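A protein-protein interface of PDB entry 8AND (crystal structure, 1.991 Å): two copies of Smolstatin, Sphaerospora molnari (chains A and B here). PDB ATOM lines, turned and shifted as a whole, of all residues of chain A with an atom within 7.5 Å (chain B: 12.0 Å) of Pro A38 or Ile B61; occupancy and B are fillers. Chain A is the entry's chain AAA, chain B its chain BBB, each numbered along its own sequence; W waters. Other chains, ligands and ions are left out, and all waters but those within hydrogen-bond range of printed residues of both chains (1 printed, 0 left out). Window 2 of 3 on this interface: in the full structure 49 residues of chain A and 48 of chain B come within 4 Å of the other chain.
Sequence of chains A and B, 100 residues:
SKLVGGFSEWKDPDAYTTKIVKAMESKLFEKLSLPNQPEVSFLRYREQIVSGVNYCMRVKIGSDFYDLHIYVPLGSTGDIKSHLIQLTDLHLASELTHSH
N of Lys B60 is in hydrogen-bond range of O of Ser A41.
The backbone carbonyl oxygen (O) of Arg B58 is in hydrogen-bond range of the backbone NH (N) of Leu A43 (2.9 Å).
The backbone carbonyl oxygen (O) of Phe A29 sits at hydrogen-bond distance from the backbone NH (N) of Leu A34 (2.8 Å).
The backbone carbonyl oxygen (O) of Met B57 is in hydrogen-bond range of the backbone NH (N) of Leu B68 (2.7 Å).
The side-chain carboxylate (OD1) of Asp B67 lies within salt-bridge range of the guanidinium group (NH2) of Arg B58, 2.8 Å away.
The backbone carbonyl oxygen (O) of Val B59 sits at hydrogen-bond distance from the backbone NH (N) of Tyr B66, at 2.7 Å.
O of Phe B65 is in hydrogen-bond range of N of Ala B93 (2.9 Å).
Among the printed residues, pairs that only touch across the chains: Ser A41 with Val B59, Leu A43 with Phe B65, Leu A28 with Leu B90, Leu A28 with Leu B68, Val A40 with Lys B60, Glu A39 with Lys B60, Pro A38 with Ile B61, Leu A32 with Leu B90, Leu A32 with Ile B61, Val A40 with Val B59, Glu A39 with Ile B61, Leu A32 with Tyr B66 and Leu A34 with Ile B61.
Of chain B, only Ile B61 (3.7 Å) comes within 4 Å of Pro A38.
Of the printed residues of chain A, Ile B61 touches Leu A32, Leu A34, Pro A38 and Glu A39.
Of the printed residues of chain B, Leu A28 touches Leu B68 and Leu B90.
No residue of chain B comes within 4 Å of Asn A36.
No residue of chain B comes within 4 Å of Gln A37.
Glu A39 touches just these residues of chain B: Lys B60 (3.7 Å) and Ile B61 (3.9 Å).
Val A40 touches just these residues of chain B: Val B59 and Lys B60.
No residue of chain A comes within 4 Å of Gly B62.
Of the printed residues of chain B, Leu A34 touches Ile B61 (3.99 Å).
Printed residues of chain A within 4 Å of Tyr B66: Leu A32 (3.98 Å).
Of the printed residues of chain A, Leu B68 touches Leu A28.
Ser B94 touches none of the printed residues of chain A.
Ala B93 touches none of the printed residues of chain A.
The nearest residue of chain B that does not touch Pro A38 is Gly B62 (5.3 Å).
Of the 13 printed residues of chain A, 8 touch a printed residue of chain B.
Printed residues of chain A that touch a printed residue of chain B: Leu A28, Leu A32, Leu A34, Pro A38, Glu A39, Val A40, Ser A41 and Leu A43.
Of the 21 printed residues of chain B, 8 touch a printed residue of chain A.
Along chain B the printed residues that touch a printed residue of chain A span positions 58 to 90.
No position is printed for both chains.
Of the 15 pairs that touch across the chains among the printed residues, none has its exchanged pair printed and touching as well.
Water W1 bridges O of Glu A39 (2.8 Å) and N of Gly B62 (2.8 Å).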
ATOM      1  N   GLU A  25      -5.899  15.591  -2.100  1.00  0.00           N
ATOM      2  CA  GLU A  25      -6.463  16.897  -1.678  1.00  0.00           C
ATOM      3  C   GLU A  25      -7.057  17.644  -2.876  1.00  0.00           C
ATOM      4  O   GLU A  25      -8.145  18.205  -2.719  1.00  0.00           O
ATOM      5  CB  GLU A  25      -5.415  17.754  -0.977  1.00  0.00           C
ATOM      6  CG  GLU A  25      -5.411  17.554   0.520  1.00  0.00           C
ATOM      7  CD  GLU A  25      -4.315  18.316   1.242  1.00  0.00           C
ATOM      8  OE1 GLU A  25      -3.572  19.093   0.592  1.00  0.00           O
ATOM      9  OE2 GLU A  25      -4.193  18.112   2.450  1.00  0.00           O
ATOM     10  N   LEU A  28     -10.342  16.169  -3.610  1.00  0.00           N
ATOM     11  CA  LEU A  28     -11.237  16.544  -2.499  1.00  0.00           C
ATOM     12  C   LEU A  28     -11.842  17.915  -2.769  1.00  0.00           C
ATOM     13  O   LEU A  28     -13.074  18.028  -2.705  1.00  0.00           O
ATOM     14  CB  LEU A  28     -10.436  16.575  -1.200  1.00  0.00           C
ATOM     15  CG  LEU A  28     -10.527  15.314  -0.375  1.00  0.00           C
ATOM     16  CD1 LEU A  28      -9.830  15.568   0.949  1.00  0.00           C
ATOM     17  CD2 LEU A  28     -11.994  14.929  -0.187  1.00  0.00           C
ATOM     18  N   PHE A  29     -10.989  18.906  -2.984  1.00  0.00           N
ATOM     19  CA  PHE A  29     -11.403  20.322  -3.086  1.00  0.00           C
ATOM     20  C   PHE A  29     -12.355  20.491  -4.268  1.00  0.00           C
ATOM     21  O   PHE A  29     -13.288  21.282  -4.210  1.00  0.00           O
ATOM     22  CB  PHE A  29     -10.173  21.210  -3.229  1.00  0.00           C
ATOM     23  CG  PHE A  29      -9.255  21.170  -2.037  1.00  0.00           C
ATOM     24  CD1 PHE A  29      -9.758  21.059  -0.748  1.00  0.00           C
ATOM     25  CD2 PHE A  29      -7.880  21.281  -2.211  1.00  0.00           C
ATOM     26  CE1 PHE A  29      -8.901  21.042   0.344  1.00  0.00           C
ATOM     27  CE2 PHE A  29      -7.022  21.251  -1.120  1.00  0.00           C
ATOM     28  CZ  PHE A  29      -7.537  21.141   0.156  1.00  0.00           C
ATOM     29  N   LEU A  32     -15.859  18.910  -3.685  1.00  0.00           N
ATOM     30  CA  LEU A  32     -16.623  19.680  -2.677  1.00  0.00           C
ATOM     31  C   LEU A  32     -16.911  21.084  -3.200  1.00  0.00           C
ATOM     32  O   LEU A  32     -17.739  21.768  -2.565  1.00  0.00           O
ATOM     33  CB  LEU A  32     -15.833  19.714  -1.363  1.00  0.00           C
ATOM     34  CG  LEU A  32     -15.860  18.397  -0.591  1.00  0.00           C
ATOM     35  CD1 LEU A  32     -14.961  18.464   0.631  1.00  0.00           C
ATOM     36  CD2 LEU A  32     -17.293  18.044  -0.194  1.00  0.00           C
ATOM     37  N   LEU A  34     -14.709  23.507  -3.176  1.00  0.00           N
ATOM     38  CA  LEU A  34     -14.022  24.377  -2.183  1.00  0.00           C
ATOM     39  C   LEU A  34     -12.772  24.949  -2.838  1.00  0.00           C
ATOM     40  O   LEU A  34     -11.771  24.248  -2.966  1.00  0.00           O
ATOM     41  CB  LEU A  34     -13.637  23.570  -0.935  1.00  0.00           C
ATOM     42  CG  LEU A  34     -14.754  22.866  -0.166  1.00  0.00           C
ATOM     43  CD1 LEU A  34     -14.211  22.350   1.161  1.00  0.00           C
ATOM     44  CD2 LEU A  34     -15.952  23.775   0.067  1.00  0.00           C
ATOM     45  N   PRO A  35     -12.771  26.233  -3.265  1.00  0.00           N
ATOM     46  CA  PRO A  35     -11.694  26.733  -4.125  1.00  0.00           C
ATOM     47  C   PRO A  35     -10.387  27.188  -3.451  1.00  0.00           C
ATOM     48  O   PRO A  35      -9.388  27.292  -4.138  1.00  0.00           O
ATOM     49  CB  PRO A  35     -12.365  27.938  -4.803  1.00  0.00           C
ATOM     50  CG  PRO A  35     -13.314  28.467  -3.744  1.00  0.00           C
ATOM     51  CD  PRO A  35     -13.818  27.241  -3.003  1.00  0.00           C
ATOM     52  N   ASN A  36     -10.406  27.440  -2.144  1.00  0.00           N
ATOM     53  CA  ASN A  36      -9.283  28.120  -1.433  1.00  0.00           C
ATOM     54  C   ASN A  36      -8.284  27.119  -0.822  1.00  0.00           C
ATOM     55  O   ASN A  36      -7.336  27.583  -0.158  1.00  0.00           O
ATOM     56  CB  ASN A  36      -9.828  29.056  -0.352  1.00  0.00           C
ATOM     57  CG  ASN A  36     -10.866  28.393   0.533  1.00  0.00           C
ATOM     58  OD1 ASN A  36     -11.768  27.705   0.043  1.00  0.00           O
ATOM     59  ND2 ASN A  36     -10.740  28.584   1.840  1.00  0.00           N
ATOM     60  N   GLN A  37      -8.478  25.811  -1.019  1.00  0.00           N
ATOM     61  CA  GLN A  37      -7.606  24.739  -0.466  1.00  0.00           C
ATOM     62  C   GLN A  37      -7.507  24.831   1.051  1.00  0.00           C
ATOM     63  O   GLN A  37      -6.408  24.943   1.581  1.00  0.00           O
ATOM     64  CB  GLN A  37      -6.196  24.856  -1.034  1.00  0.00           C
ATOM     65  CG  GLN A  37      -6.123  24.566  -2.515  1.00  0.00           C
ATOM     66  CD  GLN A  37      -4.720  24.761  -3.021  1.00  0.00           C
ATOM     67  OE1 GLN A  37      -4.239  23.998  -3.851  1.00  0.00           O
ATOM     68  NE2 GLN A  37      -4.043  25.782  -2.513  1.00  0.00           N
ATOM     69  N   PRO A  38      -8.625  24.714   1.801  1.00  0.00           N
ATOM     70  CA  PRO A  38      -8.556  24.789   3.257  1.00  0.00           C
ATOM     71  C   PRO A  38      -7.784  23.594   3.832  1.00  0.00           C
ATOM     72  O   PRO A  38      -7.516  22.598   3.122  1.00  0.00           O
ATOM     73  CB  PRO A  38     -10.019  24.748   3.690  1.00  0.00           C
ATOM     74  CG  PRO A  38     -10.697  23.972   2.592  1.00  0.00           C
ATOM     75  CD  PRO A  38      -9.976  24.381   1.323  1.00  0.00           C
ATOM     76  N   GLU A  39      -7.400  23.718   5.097  1.00  0.00           N
ATOM     77  CA  GLU A  39      -6.638  22.650   5.789  1.00  0.00           C
ATOM     78  C   GLU A  39      -7.500  21.394   5.818  1.00  0.00           C
ATOM     79  O   GLU A  39      -8.670  21.487   6.238  1.00  0.00           O
ATOM     80  CB  GLU A  39      -6.294  23.055   7.211  1.00  0.00           C
ATOM     81  CG  GLU A  39      -5.098  22.326   7.773  1.00  0.00           C
ATOM     82  CD  GLU A  39      -4.633  22.868   9.116  1.00  0.00           C
ATOM     83  OE1 GLU A  39      -4.586  24.111   9.274  1.00  0.00           O
ATOM     84  OE2 GLU A  39      -4.333  22.052  10.004  1.00  0.00           O
ATOM     85  N   VAL A  40      -6.943  20.285   5.350  1.00  0.00           N
ATOM     86  CA  VAL A  40      -7.544  18.941   5.559  1.00  0.00           C
ATOM     87  C   VAL A  40      -6.816  18.276   6.728  1.00  0.00           C
ATOM     88  O   VAL A  40      -5.602  17.975   6.589  1.00  0.00           O
ATOM     89  CB  VAL A  40      -7.464  18.096   4.285  1.00  0.00           C
ATOM     90  CG1 VAL A  40      -8.170  16.774   4.485  1.00  0.00           C
ATOM     91  CG2 VAL A  40      -8.030  18.852   3.085  1.00  0.00           C
ATOM     92  N   SER A  41      -7.516  18.069   7.835  1.00  0.00           N
ATOM     93  CA  SER A  41      -6.954  17.406   9.041  1.00  0.00           C
ATOM     94  C   SER A  41      -7.286  15.910   9.011  1.00  0.00           C
ATOM     95  O   SER A  41      -8.474  15.551   8.974  1.00  0.00           O
ATOM     96  CB  SER A  41      -7.424  18.042  10.293  1.00  0.00           C
ATOM     97  OG  SER A  41      -6.799  19.292  10.443  1.00  0.00           O
ATOM     98  N   LEU A  43      -7.491  12.429  10.734  1.00  0.00           N
ATOM     99  CA  LEU A  43      -7.713  12.051  12.147  1.00  0.00           C
ATOM    100  C   LEU A  43      -7.432  10.564  12.399  1.00  0.00           C
ATOM    101  O   LEU A  43      -6.845  10.239  13.428  1.00  0.00           O
ATOM    102  CB  LEU A  43      -9.138  12.437  12.535  1.00  0.00           C
ATOM    103  CG  LEU A  43      -9.501  13.885  12.227  1.00  0.00           C
ATOM    104  CD1 LEU A  43     -10.873  14.224  12.745  1.00  0.00           C
ATOM    105  CD2 LEU A  43      -8.480  14.852  12.799  1.00  0.00           C
ATOM    106  N   MET B  57     -10.801   7.000   5.205  1.00  0.00           N
ATOM    107  CA  MET B  57     -10.021   8.081   5.855  1.00  0.00           C
ATOM    108  C   MET B  57     -11.011   9.042   6.525  1.00  0.00           C
ATOM    109  O   MET B  57     -11.863   9.616   5.820  1.00  0.00           O
ATOM    110  CB  MET B  57      -9.141   8.817   4.827  1.00  0.00           C
ATOM    111  CG  MET B  57      -8.319   7.916   3.915  1.00  0.00           C
ATOM    112  SD  MET B  57      -7.074   6.969   4.774  1.00  0.00           S
ATOM    113  CE  MET B  57      -5.851   6.840   3.476  1.00  0.00           C
ATOM    114  N   ARG B  58     -10.882   9.230   7.843  1.00  0.00           N
ATOM    115  CA  ARG B  58     -11.653  10.259   8.580  1.00  0.00           C
ATOM    116  C   ARG B  58     -10.866  11.574   8.566  1.00  0.00           C
ATOM    117  O   ARG B  58      -9.700  11.607   9.048  1.00  0.00           O
ATOM    118  CB  ARG B  58     -11.962   9.780   9.996  1.00  0.00           C
ATOM    119  CG  ARG B  58     -12.682  10.795  10.871  1.00  0.00           C
ATOM    120  CD  ARG B  58     -14.069  11.161  10.374  1.00  0.00           C
ATOM    121  NE  ARG B  58     -14.853   9.967  10.076  1.00  0.00           N
ATOM    122  CZ  ARG B  58     -15.516   9.220  10.941  1.00  0.00           C
ATOM    123  NH1 ARG B  58     -15.518   9.487  12.232  1.00  0.00           N
ATOM    124  NH2 ARG B  58     -16.169   8.173  10.509  1.00  0.00           N
ATOM    125  N   VAL B  59     -11.470  12.625   8.029  1.00  0.00           N
ATOM    126  CA  VAL B  59     -10.772  13.928   7.854  1.00  0.00           C
ATOM    127  C   VAL B  59     -11.708  15.034   8.330  1.00  0.00           C
ATOM    128  O   VAL B  59     -12.927  14.857   8.297  1.00  0.00           O
ATOM    129  CB  VAL B  59     -10.335  14.168   6.402  1.00  0.00           C
ATOM    130  CG1 VAL B  59      -9.414  13.070   5.897  1.00  0.00           C
ATOM    131  CG2 VAL B  59     -11.545  14.318   5.489  1.00  0.00           C
ATOM    132  N   LYS B  60     -11.114  16.121   8.780  1.00  0.00           N
ATOM    133  CA  LYS B  60     -11.848  17.350   9.137  1.00  0.00           C
ATOM    134  C   LYS B  60     -11.490  18.409   8.107  1.00  0.00           C
ATOM    135  O   LYS B  60     -10.276  18.620   7.852  1.00  0.00           O
ATOM    136  CB  LYS B  60     -11.513  17.812  10.553  1.00  0.00           C
ATOM    137  CG  LYS B  60     -12.364  18.973  11.034  1.00  0.00           C
ATOM    138  CD  LYS B  60     -11.965  19.486  12.374  1.00  0.00           C
ATOM    139  CE  LYS B  60     -13.078  20.326  12.980  1.00  0.00           C
ATOM    140  NZ  LYS B  60     -12.576  21.176  14.076  1.00  0.00           N
ATOM    141  N   ILE B  61     -12.518  18.984   7.485  1.00  0.00           N
ATOM    142  CA  ILE B  61     -12.380  20.203   6.634  1.00  0.00           C
ATOM    143  C   ILE B  61     -13.364  21.258   7.150  1.00  0.00           C
ATOM    144  O   ILE B  61     -14.578  20.971   7.231  1.00  0.00           O
ATOM    145  CB  ILE B  61     -12.613  19.866   5.155  1.00  0.00           C
ATOM    146  CG1 ILE B  61     -11.963  18.532   4.810  1.00  0.00           C
ATOM    147  CG2 ILE B  61     -12.097  20.990   4.260  1.00  0.00           C
ATOM    148  CD1 ILE B  61     -12.357  17.985   3.466  1.00  0.00           C
ATOM    149  N   GLY B  62     -12.845  22.433   7.495  1.00  0.00           N
ATOM    150  CA  GLY B  62     -13.667  23.464   8.146  1.00  0.00           C
ATOM    151  C   GLY B  62     -14.082  22.966   9.512  1.00  0.00           C
ATOM    152  O   GLY B  62     -13.219  22.445  10.241  1.00  0.00           O
ATOM    153  N   SER B  63     -15.374  23.046   9.825  1.00  0.00           N
ATOM    154  CA  SER B  63     -15.958  22.474  11.061  1.00  0.00           C
ATOM    155  C   SER B  63     -16.673  21.152  10.784  1.00  0.00           C
ATOM    156  O   SER B  63     -17.322  20.658  11.724  1.00  0.00           O
ATOM    157  CB  SER B  63     -16.891  23.471  11.704  1.00  0.00           C
ATOM    158  OG  SER B  63     -17.997  23.774  10.853  1.00  0.00           O
ATOM    159  N   ASP B  64     -16.514  20.576   9.580  1.00  0.00           N
ATOM    160  CA  ASP B  64     -17.221  19.337   9.154  1.00  0.00           C
ATOM    161  C   ASP B  64     -16.268  18.141   9.096  1.00  0.00           C
ATOM    162  O   ASP B  64     -15.063  18.302   8.797  1.00  0.00           O
ATOM    163  CB  ASP B  64     -17.924  19.536   7.813  1.00  0.00           C
ATOM    164  CG  ASP B  64     -19.159  20.406   7.934  1.00  0.00           C
ATOM    165  OD1 ASP B  64     -19.992  20.099   8.787  1.00  0.00           O
ATOM    166  OD2 ASP B  64     -19.232  21.387   7.218  1.00  0.00           O
ATOM    167  N   PHE B  65     -16.804  16.967   9.373  1.00  0.00           N
ATOM    168  CA  PHE B  65     -16.028  15.710   9.395  1.00  0.00           C
ATOM    169  C   PHE B  65     -16.465  14.860   8.211  1.00  0.00           C
ATOM    170  O   PHE B  65     -17.724  14.744   7.959  1.00  0.00           O
ATOM    171  CB  PHE B  65     -16.216  14.996  10.728  1.00  0.00           C
ATOM    172  CG  PHE B  65     -15.545  15.688  11.885  1.00  0.00           C
ATOM    173  CD1 PHE B  65     -14.214  15.448  12.195  1.00  0.00           C
ATOM    174  CD2 PHE B  65     -16.242  16.597  12.646  1.00  0.00           C
ATOM    175  CE1 PHE B  65     -13.597  16.125  13.239  1.00  0.00           C
ATOM    176  CE2 PHE B  65     -15.631  17.266  13.695  1.00  0.00           C
ATOM    177  CZ  PHE B  65     -14.311  17.023  13.993  1.00  0.00           C
ATOM    178  N   TYR B  66     -15.494  14.296   7.494  1.00  0.00           N
ATOM    179  CA  TYR B  66     -15.803  13.474   6.289  1.00  0.00           C
ATOM    180  C   TYR B  66     -15.230  12.067   6.371  1.00  0.00           C
ATOM    181  O   TYR B  66     -14.194  11.808   7.041  1.00  0.00           O
ATOM    182  CB  TYR B  66     -15.292  14.144   5.015  1.00  0.00           C
ATOM    183  CG  TYR B  66     -15.904  15.487   4.744  1.00  0.00           C
ATOM    184  CD1 TYR B  66     -15.454  16.619   5.397  1.00  0.00           C
ATOM    185  CD2 TYR B  66     -16.929  15.629   3.826  1.00  0.00           C
ATOM    186  CE1 TYR B  66     -16.016  17.857   5.159  1.00  0.00           C
ATOM    187  CE2 TYR B  66     -17.531  16.856   3.599  1.00  0.00           C
ATOM    188  CZ  TYR B  66     -17.071  17.973   4.266  1.00  0.00           C
ATOM    189  OH  TYR B  66     -17.596  19.207   4.018  1.00  0.00           O
ATOM    190  N   ASP B  67     -15.899  11.152   5.675  1.00  0.00           N
ATOM    191  CA  ASP B  67     -15.329   9.837   5.321  1.00  0.00           C
ATOM    192  C   ASP B  67     -14.823   9.888   3.879  1.00  0.00           C
ATOM    193  O   ASP B  67     -15.650  10.037   2.959  1.00  0.00           O
ATOM    194  CB  ASP B  67     -16.339   8.697   5.491  1.00  0.00           C
ATOM    195  CG  ASP B  67     -16.592   8.283   6.937  1.00  0.00           C
ATOM    196  OD1 ASP B  67     -15.772   8.619   7.809  1.00  0.00           O
ATOM    197  OD2 ASP B  67     -17.595   7.592   7.171  1.00  0.00           O
ATOM    198  N   LEU B  68     -13.520   9.722   3.695  1.00  0.00           N
ATOM    199  CA  LEU B  68     -12.860   9.649   2.360  1.00  0.00           C
ATOM    200  C   LEU B  68     -12.633   8.184   2.037  1.00  0.00           C
ATOM    201  O   LEU B  68     -11.750   7.571   2.667  1.00  0.00           O
ATOM    202  CB  LEU B  68     -11.489  10.342   2.413  1.00  0.00           C
ATOM    203  CG  LEU B  68     -11.268  11.692   1.757  1.00  0.00           C
ATOM    204  CD1 LEU B  68     -11.922  12.777   2.581  1.00  0.00           C
ATOM    205  CD2 LEU B  68      -9.763  11.953   1.658  1.00  0.00           C
ATOM    206  N   HIS B  69     -13.398   7.634   1.104  1.00  0.00           N
ATOM    207  CA  HIS B  69     -13.206   6.230   0.660  1.00  0.00           C
ATOM    208  C   HIS B  69     -12.221   6.258  -0.503  1.00  0.00           C
ATOM    209  O   HIS B  69     -12.505   6.911  -1.550  1.00  0.00           O
ATOM    210  CB  HIS B  69     -14.527   5.581   0.280  1.00  0.00           C
ATOM    211  CG  HIS B  69     -15.492   5.452   1.405  1.00  0.00           C
ATOM    212  ND1 HIS B  69     -15.594   4.291   2.161  1.00  0.00           N
ATOM    213  CD2 HIS B  69     -16.422   6.302   1.890  1.00  0.00           C
ATOM    214  CE1 HIS B  69     -16.540   4.443   3.068  1.00  0.00           C
ATOM    215  NE2 HIS B  69     -17.065   5.665   2.924  1.00  0.00           N
ATOM    216  N   ILE B  70     -11.080   5.632  -0.308  1.00  0.00           N
ATOM    217  CA  ILE B  70      -9.952   5.705  -1.279  1.00  0.00           C
ATOM    218  C   ILE B  70      -9.509   4.291  -1.596  1.00  0.00           C
ATOM    219  O   ILE B  70      -9.436   3.450  -0.674  1.00  0.00           O
ATOM    220  CB  ILE B  70      -8.806   6.552  -0.727  1.00  0.00           C
ATOM    221  CG1 ILE B  70      -9.222   8.021  -0.648  1.00  0.00           C
ATOM    222  CG2 ILE B  70      -7.547   6.358  -1.550  1.00  0.00           C
ATOM    223  CD1 ILE B  70      -8.276   8.884   0.167  1.00  0.00           C
ATOM    224  N   LEU B  87     -10.391   8.120  -5.697  1.00  0.00           N
ATOM    225  CA  LEU B  87     -11.301   8.671  -4.678  1.00  0.00           C
ATOM    226  C   LEU B  87     -12.674   8.073  -4.984  1.00  0.00           C
ATOM    227  O   LEU B  87     -13.372   8.565  -5.878  1.00  0.00           O
ATOM    228  CB  LEU B  87     -11.293  10.204  -4.714  1.00  0.00           C
ATOM    229  CG  LEU B  87     -12.289  10.886  -3.770  1.00  0.00           C
ATOM    230  CD1 LEU B  87     -12.210  10.249  -2.404  1.00  0.00           C
ATOM    231  CD2 LEU B  87     -12.048  12.388  -3.656  1.00  0.00           C
ATOM    232  N   ASP B  89     -15.364   7.413  -3.022  1.00  0.00           N
ATOM    233  CA  ASP B  89     -16.567   8.012  -2.404  1.00  0.00           C
ATOM    234  C   ASP B  89     -16.156   9.071  -1.389  1.00  0.00           C
ATOM    235  O   ASP B  89     -15.016   9.028  -0.874  1.00  0.00           O
ATOM    236  CB  ASP B  89     -17.467   6.944  -1.783  1.00  0.00           C
ATOM    237  CG  ASP B  89     -18.896   7.428  -1.631  1.00  0.00           C
ATOM    238  OD1 ASP B  89     -19.236   8.444  -2.269  1.00  0.00           O
ATOM    239  OD2 ASP B  89     -19.641   6.813  -0.855  1.00  0.00           O
ATOM    240  N   LEU B  90     -17.056  10.010  -1.146  1.00  0.00           N
ATOM    241  CA  LEU B  90     -16.830  11.083  -0.166  1.00  0.00           C
ATOM    242  C   LEU B  90     -18.170  11.520   0.408  1.00  0.00           C
ATOM    243  O   LEU B  90     -19.068  11.852  -0.368  1.00  0.00           O
ATOM    244  CB  LEU B  90     -16.140  12.247  -0.869  1.00  0.00           C
ATOM    245  CG  LEU B  90     -15.888  13.465   0.008  1.00  0.00           C
ATOM    246  CD1 LEU B  90     -14.753  13.200   0.988  1.00  0.00           C
ATOM    247  CD2 LEU B  90     -15.578  14.667  -0.857  1.00  0.00           C
ATOM    248  N   HIS B  91     -18.291  11.535   1.728  1.00  0.00           N
ATOM    249  CA  HIS B  91     -19.544  11.994   2.380  1.00  0.00           C
ATOM    250  C   HIS B  91     -19.262  12.452   3.809  1.00  0.00           C
ATOM    251  O   HIS B  91     -18.214  12.055   4.400  1.00  0.00           O
ATOM    252  CB  HIS B  91     -20.618  10.900   2.315  1.00  0.00           C
ATOM    253  CG  HIS B  91     -20.213   9.594   2.900  1.00  0.00           C
ATOM    254  ND1 HIS B  91     -20.222   9.360   4.264  1.00  0.00           N
ATOM    255  CD2 HIS B  91     -19.804   8.442   2.321  1.00  0.00           C
ATOM    256  CE1 HIS B  91     -19.831   8.118   4.498  1.00  0.00           C
ATOM    257  NE2 HIS B  91     -19.561   7.533   3.321  1.00  0.00           N
ATOM    258  N   LEU B  92     -20.176  13.259   4.340  1.00  0.00           N
ATOM    259  CA  LEU B  92     -20.129  13.633   5.766  1.00  0.00           C
ATOM    260  C   LEU B  92     -20.115  12.353   6.597  1.00  0.00           C
ATOM    261  O   LEU B  92     -20.893  11.429   6.293  1.00  0.00           O
ATOM    262  CB  LEU B  92     -21.323  14.510   6.129  1.00  0.00           C
ATOM    263  CG  LEU B  92     -21.328  15.911   5.532  1.00  0.00           C
ATOM    264  CD1 LEU B  92     -22.681  16.578   5.752  1.00  0.00           C
ATOM    265  CD2 LEU B  92     -20.219  16.758   6.135  1.00  0.00           C
ATOM    266  N   ALA B  93     -19.219  12.293   7.587  1.00  0.00           N
ATOM    267  CA  ALA B  93     -19.128  11.142   8.505  1.00  0.00           C
ATOM    268  C   ALA B  93     -20.511  10.827   9.091  1.00  0.00           C
ATOM    269  O   ALA B  93     -20.716   9.687   9.519  1.00  0.00           O
ATOM    270  CB  ALA B  93     -18.123  11.425   9.574  1.00  0.00           C
ATOM    271  N   SER B  94     -21.428  11.795   9.087  1.00  0.00           N
ATOM    272  CA  SER B  94     -22.835  11.624   9.533  1.00  0.00           C
ATOM    273  C   SER B  94     -23.591  10.698   8.568  1.00  0.00           C
ATOM    274  O   SER B  94     -24.278   9.772   9.003  1.00  0.00           O
ATOM    275  CB  SER B  94     -23.516  12.961   9.654  1.00  0.00           C
ATOM    276  OG  SER B  94     -22.862  13.790  10.597  1.00  0.00           O
HETATM  277  O   HOH W   1     -10.322  23.606   7.065  1.00  0.00           O
